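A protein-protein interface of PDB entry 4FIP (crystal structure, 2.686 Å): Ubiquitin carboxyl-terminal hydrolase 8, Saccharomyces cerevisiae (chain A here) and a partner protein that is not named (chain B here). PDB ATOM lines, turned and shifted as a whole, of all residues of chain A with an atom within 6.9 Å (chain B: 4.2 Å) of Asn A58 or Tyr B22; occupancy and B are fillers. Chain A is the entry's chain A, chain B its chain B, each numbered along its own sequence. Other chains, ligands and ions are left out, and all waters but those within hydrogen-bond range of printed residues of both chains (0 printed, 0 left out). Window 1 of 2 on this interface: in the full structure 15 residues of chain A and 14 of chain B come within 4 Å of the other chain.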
ATOM      1  N   PHE A  45      -7.620 -25.911  -8.436  1.00  0.00           N
ATOM      2  CA  PHE A  45      -6.635 -25.840  -9.490  1.00  0.00           C
ATOM      3  C   PHE A  45      -6.029 -27.213  -9.785  1.00  0.00           C
ATOM      4  O   PHE A  45      -5.786 -27.516 -10.949  1.00  0.00           O
ATOM      5  CB  PHE A  45      -5.519 -24.862  -9.175  1.00  0.00           C
ATOM      6  CG  PHE A  45      -5.929 -23.426  -9.198  1.00  0.00           C
ATOM      7  CD1 PHE A  45      -6.457 -22.860 -10.333  1.00  0.00           C
ATOM      8  CD2 PHE A  45      -5.726 -22.620  -8.107  1.00  0.00           C
ATOM      9  CE1 PHE A  45      -6.825 -21.526 -10.370  1.00  0.00           C
ATOM     10  CE2 PHE A  45      -6.092 -21.277  -8.122  1.00  0.00           C
ATOM     11  CZ  PHE A  45      -6.643 -20.726  -9.260  1.00  0.00           C
ATOM     12  N   THR A  48      -9.451 -30.167 -10.718  1.00  0.00           N
ATOM     13  CA  THR A  48     -10.425 -29.855 -11.757  1.00  0.00           C
ATOM     14  C   THR A  48      -9.956 -28.898 -12.851  1.00  0.00           C
ATOM     15  O   THR A  48     -10.734 -28.611 -13.743  1.00  0.00           O
ATOM     16  CB  THR A  48     -11.634 -29.207 -11.160  1.00  0.00           C
ATOM     17  OG1 THR A  48     -11.269 -27.905 -10.715  1.00  0.00           O
ATOM     18  CG2 THR A  48     -12.129 -30.032 -10.005  1.00  0.00           C
ATOM     19  N   MET A  49      -8.721 -28.381 -12.795  1.00  0.00           N
ATOM     20  CA  MET A  49      -8.231 -27.461 -13.852  1.00  0.00           C
ATOM     21  C   MET A  49      -6.876 -27.916 -14.358  1.00  0.00           C
ATOM     22  O   MET A  49      -6.084 -27.105 -14.878  1.00  0.00           O
ATOM     23  CB  MET A  49      -8.175 -25.991 -13.361  1.00  0.00           C
ATOM     24  CG  MET A  49      -9.539 -25.336 -13.182  1.00  0.00           C
ATOM     25  SD  MET A  49      -9.614 -23.954 -12.023  1.00  0.00           S
ATOM     26  CE  MET A  49     -11.390 -23.586 -12.016  1.00  0.00           C
ATOM     27  N   LYS A  50      -6.620 -29.219 -14.208  1.00  0.00           N
ATOM     28  CA  LYS A  50      -5.355 -29.799 -14.588  1.00  0.00           C
ATOM     29  C   LYS A  50      -5.674 -30.880 -15.581  1.00  0.00           C
ATOM     30  O   LYS A  50      -6.409 -31.835 -15.279  1.00  0.00           O
ATOM     31  CB  LYS A  50      -4.641 -30.393 -13.389  1.00  0.00           C
ATOM     32  CG  LYS A  50      -3.321 -31.101 -13.706  1.00  0.00           C
ATOM     33  CD  LYS A  50      -2.545 -31.436 -12.439  1.00  0.00           C
ATOM     34  CE  LYS A  50      -1.432 -32.445 -12.666  1.00  0.00           C
ATOM     35  NZ  LYS A  50      -1.032 -33.065 -11.363  1.00  0.00           N
ATOM     36  N   CYS A  51      -5.134 -30.687 -16.774  1.00  0.00           N
ATOM     37  CA  CYS A  51      -5.378 -31.573 -17.874  1.00  0.00           C
ATOM     38  C   CYS A  51      -4.790 -32.939 -17.540  1.00  0.00           C
ATOM     39  O   CYS A  51      -3.643 -33.035 -17.138  1.00  0.00           O
ATOM     40  CB  CYS A  51      -4.707 -30.992 -19.112  1.00  0.00           C
ATOM     41  SG  CYS A  51      -5.133 -31.823 -20.626  1.00  0.00           S
ATOM     42  N   GLU A  56      -0.988 -29.612 -17.555  1.00  0.00           N
ATOM     43  CA  GLU A  56      -0.967 -28.149 -17.409  1.00  0.00           C
ATOM     44  C   GLU A  56      -2.216 -27.632 -16.657  1.00  0.00           C
ATOM     45  O   GLU A  56      -3.325 -28.209 -16.704  1.00  0.00           O
ATOM     46  CB  GLU A  56      -0.924 -27.444 -18.778  1.00  0.00           C
ATOM     47  CG  GLU A  56       0.437 -27.259 -19.437  1.00  0.00           C
ATOM     48  CD  GLU A  56       0.364 -26.367 -20.692  1.00  0.00           C
ATOM     49  OE1 GLU A  56      -0.396 -25.375 -20.711  1.00  0.00           O
ATOM     50  OE2 GLU A  56       1.060 -26.625 -21.689  1.00  0.00           O
ATOM     51  N   ILE A  57      -2.030 -26.500 -15.993  1.00  0.00           N
ATOM     52  CA  ILE A  57      -3.131 -25.831 -15.325  1.00  0.00           C
ATOM     53  C   ILE A  57      -3.657 -24.686 -16.191  1.00  0.00           C
ATOM     54  O   ILE A  57      -2.883 -23.815 -16.620  1.00  0.00           O
ATOM     55  CB  ILE A  57      -2.701 -25.381 -13.935  1.00  0.00           C
ATOM     56  CG1 ILE A  57      -2.225 -26.631 -13.185  1.00  0.00           C
ATOM     57  CG2 ILE A  57      -3.864 -24.718 -13.230  1.00  0.00           C
ATOM     58  CD1 ILE A  57      -1.588 -26.370 -11.847  1.00  0.00           C
ATOM     59  N   ASN A  58      -4.956 -24.750 -16.493  1.00  0.00           N
ATOM     60  CA  ASN A  58      -5.652 -23.714 -17.240  1.00  0.00           C
ATOM     61  C   ASN A  58      -5.192 -23.562 -18.703  1.00  0.00           C
ATOM     62  O   ASN A  58      -5.072 -22.443 -19.239  1.00  0.00           O
ATOM     63  CB  ASN A  58      -5.530 -22.367 -16.532  1.00  0.00           C
ATOM     64  CG  ASN A  58      -6.297 -22.310 -15.236  1.00  0.00           C
ATOM     65  OD1 ASN A  58      -5.837 -21.699 -14.287  1.00  0.00           O
ATOM     66  ND2 ASN A  58      -7.484 -22.913 -15.200  1.00  0.00           N
ATOM     67  N   SER A  59      -4.972 -24.693 -19.367  1.00  0.00           N
ATOM     68  CA  SER A  59      -4.682 -24.688 -20.776  1.00  0.00           C
ATOM     69  C   SER A  59      -5.996 -24.371 -21.475  1.00  0.00           C
ATOM     70  O   SER A  59      -6.520 -25.185 -22.246  1.00  0.00           O
ATOM     71  CB  SER A  59      -4.118 -26.053 -21.190  1.00  0.00           C
ATOM     72  OG  SER A  59      -3.847 -26.094 -22.582  1.00  0.00           O
ATOM     73  N   GLY A  60      -6.531 -23.187 -21.202  1.00  0.00           N
ATOM     74  CA  GLY A  60      -7.961 -22.913 -21.457  1.00  0.00           C
ATOM     75  C   GLY A  60      -8.876 -23.546 -20.408  1.00  0.00           C
ATOM     76  O   GLY A  60      -8.426 -24.037 -19.361  1.00  0.00           O
ATOM     77  N   ALA A  61     -10.176 -23.541 -20.683  1.00  0.00           N
ATOM     78  CA  ALA A  61     -11.123 -24.267 -19.845  1.00  0.00           C
ATOM     79  C   ALA A  61     -10.647 -25.687 -19.705  1.00  0.00           C
ATOM     80  O   ALA A  61     -10.059 -26.229 -20.621  1.00  0.00           O
ATOM     81  CB  ALA A  61     -12.492 -24.259 -20.471  1.00  0.00           C
ATOM     82  N   THR A  62     -10.874 -26.291 -18.554  1.00  0.00           N
ATOM     83  CA  THR A  62     -10.673 -27.699 -18.394  1.00  0.00           C
ATOM     84  C   THR A  62     -12.064 -28.279 -18.197  1.00  0.00           C
ATOM     85  O   THR A  62     -12.866 -27.680 -17.551  1.00  0.00           O
ATOM     86  CB  THR A  62      -9.753 -27.909 -17.185  1.00  0.00           C
ATOM     87  OG1 THR A  62      -8.505 -27.259 -17.449  1.00  0.00           O
ATOM     88  CG2 THR A  62      -9.505 -29.390 -16.881  1.00  0.00           C
ATOM     89  N   CYS A  73      -8.024 -30.416 -21.117  1.00  0.00           N
ATOM     90  CA  CYS A  73      -7.942 -29.014 -21.586  1.00  0.00           C
ATOM     91  C   CYS A  73      -8.581 -28.790 -22.914  1.00  0.00           C
ATOM     92  O   CYS A  73      -8.798 -29.724 -23.657  1.00  0.00           O
ATOM     93  CB  CYS A  73      -6.483 -28.526 -21.674  1.00  0.00           C
ATOM     94  SG  CYS A  73      -5.476 -29.211 -23.018  1.00  0.00           S
ATOM     95  N   ASN A  75      -7.328 -25.936 -24.989  1.00  0.00           N
ATOM     96  CA  ASN A  75      -6.362 -25.360 -25.943  1.00  0.00           C
ATOM     97  C   ASN A  75      -5.557 -26.378 -26.797  1.00  0.00           C
ATOM     98  O   ASN A  75      -5.250 -26.097 -27.932  1.00  0.00           O
ATOM     99  CB  ASN A  75      -5.418 -24.389 -25.236  1.00  0.00           C
ATOM    100  CG  ASN A  75      -6.113 -23.144 -24.728  1.00  0.00           C
ATOM    101  OD1 ASN A  75      -5.482 -22.300 -24.096  1.00  0.00           O
ATOM    102  ND2 ASN A  75      -7.411 -23.019 -24.995  1.00  0.00           N
ATOM    103  N   SER A  94     -15.003 -26.411 -15.644  1.00  0.00           N
ATOM    104  CA  SER A  94     -14.710 -26.347 -14.202  1.00  0.00           C
ATOM    105  C   SER A  94     -14.683 -24.927 -13.655  1.00  0.00           C
ATOM    106  O   SER A  94     -14.622 -24.774 -12.459  1.00  0.00           O
ATOM    107  CB  SER A  94     -13.373 -27.042 -13.878  1.00  0.00           C
ATOM    108  OG  SER A  94     -12.274 -26.290 -14.383  1.00  0.00           O
ATOM    109  N   ASN A  95     -14.713 -23.913 -14.524  1.00  0.00           N
ATOM    110  CA  ASN A  95     -14.888 -22.529 -14.109  1.00  0.00           C
ATOM    111  C   ASN A  95     -16.337 -22.139 -13.929  1.00  0.00           C
ATOM    112  O   ASN A  95     -16.586 -21.153 -13.302  1.00  0.00           O
ATOM    113  CB  ASN A  95     -14.355 -21.550 -15.151  1.00  0.00           C
ATOM    114  CG  ASN A  95     -12.849 -21.576 -15.285  1.00  0.00           C
ATOM    115  OD1 ASN A  95     -12.144 -21.232 -14.350  1.00  0.00           O
ATOM    116  ND2 ASN A  95     -12.346 -21.943 -16.473  1.00  0.00           N
ATOM    117  N   LEU B  16       3.756 -23.157  -8.309  1.00  0.00           N
ATOM    118  CA  LEU B  16       3.023 -21.920  -8.056  1.00  0.00           C
ATOM    119  C   LEU B  16       1.716 -22.203  -7.352  1.00  0.00           C
ATOM    120  O   LEU B  16       1.383 -21.568  -6.352  1.00  0.00           O
ATOM    121  CB  LEU B  16       2.712 -21.184  -9.358  1.00  0.00           C
ATOM    122  CG  LEU B  16       3.893 -20.638 -10.163  1.00  0.00           C
ATOM    123  CD1 LEU B  16       3.414 -20.290 -11.565  1.00  0.00           C
ATOM    124  CD2 LEU B  16       4.578 -19.448  -9.496  1.00  0.00           C
ATOM    125  N   VAL B  17       0.979 -23.171  -7.861  1.00  0.00           N
ATOM    126  CA  VAL B  17      -0.266 -23.496  -7.234  1.00  0.00           C
ATOM    127  C   VAL B  17      -0.048 -23.838  -5.778  1.00  0.00           C
ATOM    128  O   VAL B  17      -0.752 -23.315  -4.936  1.00  0.00           O
ATOM    129  CB  VAL B  17      -1.012 -24.628  -7.931  1.00  0.00           C
ATOM    130  CG1 VAL B  17      -1.995 -25.262  -6.971  1.00  0.00           C
ATOM    131  CG2 VAL B  17      -1.740 -24.078  -9.141  1.00  0.00           C
ATOM    132  N   GLY B  20       0.914 -21.034  -3.269  1.00  0.00           N
ATOM    133  CA  GLY B  20      -0.123 -20.027  -3.105  1.00  0.00           C
ATOM    134  C   GLY B  20       0.000 -18.833  -4.043  1.00  0.00           C
ATOM    135  O   GLY B  20      -0.898 -17.981  -4.089  1.00  0.00           O
ATOM    136  N   ASN B  21       1.081 -18.768  -4.812  1.00  0.00           N
ATOM    137  CA  ASN B  21       1.314 -17.619  -5.683  1.00  0.00           C
ATOM    138  C   ASN B  21       0.549 -17.717  -7.016  1.00  0.00           C
ATOM    139  O   ASN B  21       0.456 -16.749  -7.765  1.00  0.00           O
ATOM    140  CB  ASN B  21       2.827 -17.412  -5.879  1.00  0.00           C
ATOM    141  CG  ASN B  21       3.600 -17.339  -4.544  1.00  0.00           C
ATOM    142  OD1 ASN B  21       3.123 -16.753  -3.561  1.00  0.00           O
ATOM    143  ND2 ASN B  21       4.790 -17.941  -4.509  1.00  0.00           N
ATOM    144  N   TYR B  22      -0.031 -18.872  -7.310  1.00  0.00           N
ATOM    145  CA  TYR B  22      -0.905 -18.962  -8.463  1.00  0.00           C
ATOM    146  C   TYR B  22      -2.225 -18.244  -8.135  1.00  0.00           C
ATOM    147  O   TYR B  22      -2.575 -17.309  -8.847  1.00  0.00           O
ATOM    148  CB  TYR B  22      -1.106 -20.407  -8.907  1.00  0.00           C
ATOM    149  CG  TYR B  22      -1.658 -20.539 -10.311  1.00  0.00           C
ATOM    150  CD1 TYR B  22      -0.843 -20.335 -11.425  1.00  0.00           C
ATOM    151  CD2 TYR B  22      -3.003 -20.880 -10.531  1.00  0.00           C
ATOM    152  CE1 TYR B  22      -1.346 -20.453 -12.714  1.00  0.00           C
ATOM    153  CE2 TYR B  22      -3.515 -21.012 -11.815  1.00  0.00           C
ATOM    154  CZ  TYR B  22      -2.682 -20.799 -12.906  1.00  0.00           C
ATOM    155  OH  TYR B  22      -3.182 -20.924 -14.191  1.00  0.00           O
ATOM    156  N   GLU B  23      -2.919 -18.615  -7.047  1.00  0.00           N
ATOM    157  CA  GLU B  23      -4.027 -17.781  -6.534  1.00  0.00           C
ATOM    158  C   GLU B  23      -3.718 -16.282  -6.709  1.00  0.00           C
ATOM    159  O   GLU B  23      -4.499 -15.566  -7.332  1.00  0.00           O
ATOM    160  CB  GLU B  23      -4.344 -18.024  -5.050  1.00  0.00           C
ATOM    161  CG  GLU B  23      -5.078 -19.305  -4.694  1.00  0.00           C
ATOM    162  CD  GLU B  23      -4.161 -20.341  -4.020  1.00  0.00           C
ATOM    163  OE1 GLU B  23      -3.234 -20.920  -4.703  1.00  0.00           O
ATOM    164  OE2 GLU B  23      -4.355 -20.571  -2.788  1.00  0.00           O
ATOM    165  N   LEU B  24      -2.589 -15.823  -6.167  1.00  0.00           N
ATOM    166  CA  LEU B  24      -2.208 -14.393  -6.207  1.00  0.00           C
ATOM    167  C   LEU B  24      -2.146 -13.862  -7.644  1.00  0.00           C
ATOM    168  O   LEU B  24      -2.798 -12.882  -7.992  1.00  0.00           O
ATOM    169  CB  LEU B  24      -0.855 -14.119  -5.488  1.00  0.00           C
ATOM    170  CG  LEU B  24      -0.806 -14.018  -3.927  1.00  0.00           C
ATOM    171  CD1 LEU B  24       0.577 -14.303  -3.341  1.00  0.00           C
ATOM    172  CD2 LEU B  24      -1.287 -12.673  -3.390  1.00  0.00           C
ATOM    173  N   ILE B  25      -1.358 -14.498  -8.486  1.00  0.00           N
ATOM    174  CA  ILE B  25      -1.222 -14.002  -9.840  1.00  0.00           C
ATOM    175  C   ILE B  25      -2.593 -13.904 -10.454  1.00  0.00           C
ATOM    176  O   ILE B  25      -2.958 -12.872 -11.028  1.00  0.00           O
ATOM    177  CB  ILE B  25      -0.418 -14.953 -10.728  1.00  0.00           C
ATOM    178  CG1 ILE B  25       1.046 -14.967 -10.315  1.00  0.00           C
ATOM    179  CG2 ILE B  25      -0.532 -14.526 -12.174  1.00  0.00           C
ATOM    180  CD1 ILE B  25       1.687 -16.311 -10.578  1.00  0.00           C
ATOM    181  N   SER B  26      -3.328 -15.010 -10.318  1.00  0.00           N
ATOM    182  CA  SER B  26      -4.622 -15.191 -10.934  1.00  0.00           C
ATOM    183  C   SER B  26      -5.601 -14.137 -10.426  1.00  0.00           C
ATOM    184  O   SER B  26      -6.328 -13.523 -11.197  1.00  0.00           O
ATOM    185  CB  SER B  26      -5.138 -16.608 -10.644  1.00  0.00           C
ATOM    186  OG  SER B  26      -6.492 -16.764 -11.035  1.00  0.00           O
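Of the 16 printed residues of chain A, 3 touch a printed residue of chain B. Printed residues of chain A that touch a printed residue of chain B: Phe A45, Ile A57 and Asn A58. Of the 9 printed residues of chain B, 2 touch a printed residue of chain A. Hydrophobic or aromatic side chains of chain B within 4 Å of the printed part of chain A: Val B17 and Tyr B22. Among the printed residues, no Asp or Glu carboxylate lies within 4 Å of a Lys or Arg side-chain nitrogen of the other chain.
The side-chain hydroxyl (OH) of Tyr B22 is in hydrogen-bond range of the side-chain amide oxygen (OD1) of Asn A58 (2.8 Å).
Of the printed residues of chain B, Phe A45 touches Val B17 (3.9 Å) and Tyr B22 (3.6 Å). Of the printed residues of chain B, Ile A57 touches Val B17 and Tyr B22. Tyr B22 touches three residues of chain A. The nearest printed residue of chain B that does not touch Asn A58 is Ser B26 (5.9 Å). The nearest residue of chain A that does not touch Tyr B22 is Ser A59 (6.6 Å). The nearest printed residue of chain B that does not touch Ile A57 is Leu B16 (7.0 Å).
Val B17 touches Phe A45 (CG2 to CB, 3.9 Å). Tyr B22 touches Phe A45. Ile A57 touches Val B17. O of Ile A57 touches OH of Tyr B22, at 3.8 Å.
The backbone NH (N) of Tyr B22 is in hydrogen-bond range of the backbone carbonyl oxygen (O) of Leu B16 (3.2 Å). The backbone carbonyl oxygen of Met A49 lies within hydrogen-bond range of the backbone NH of Asn A58 (3.1 Å).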
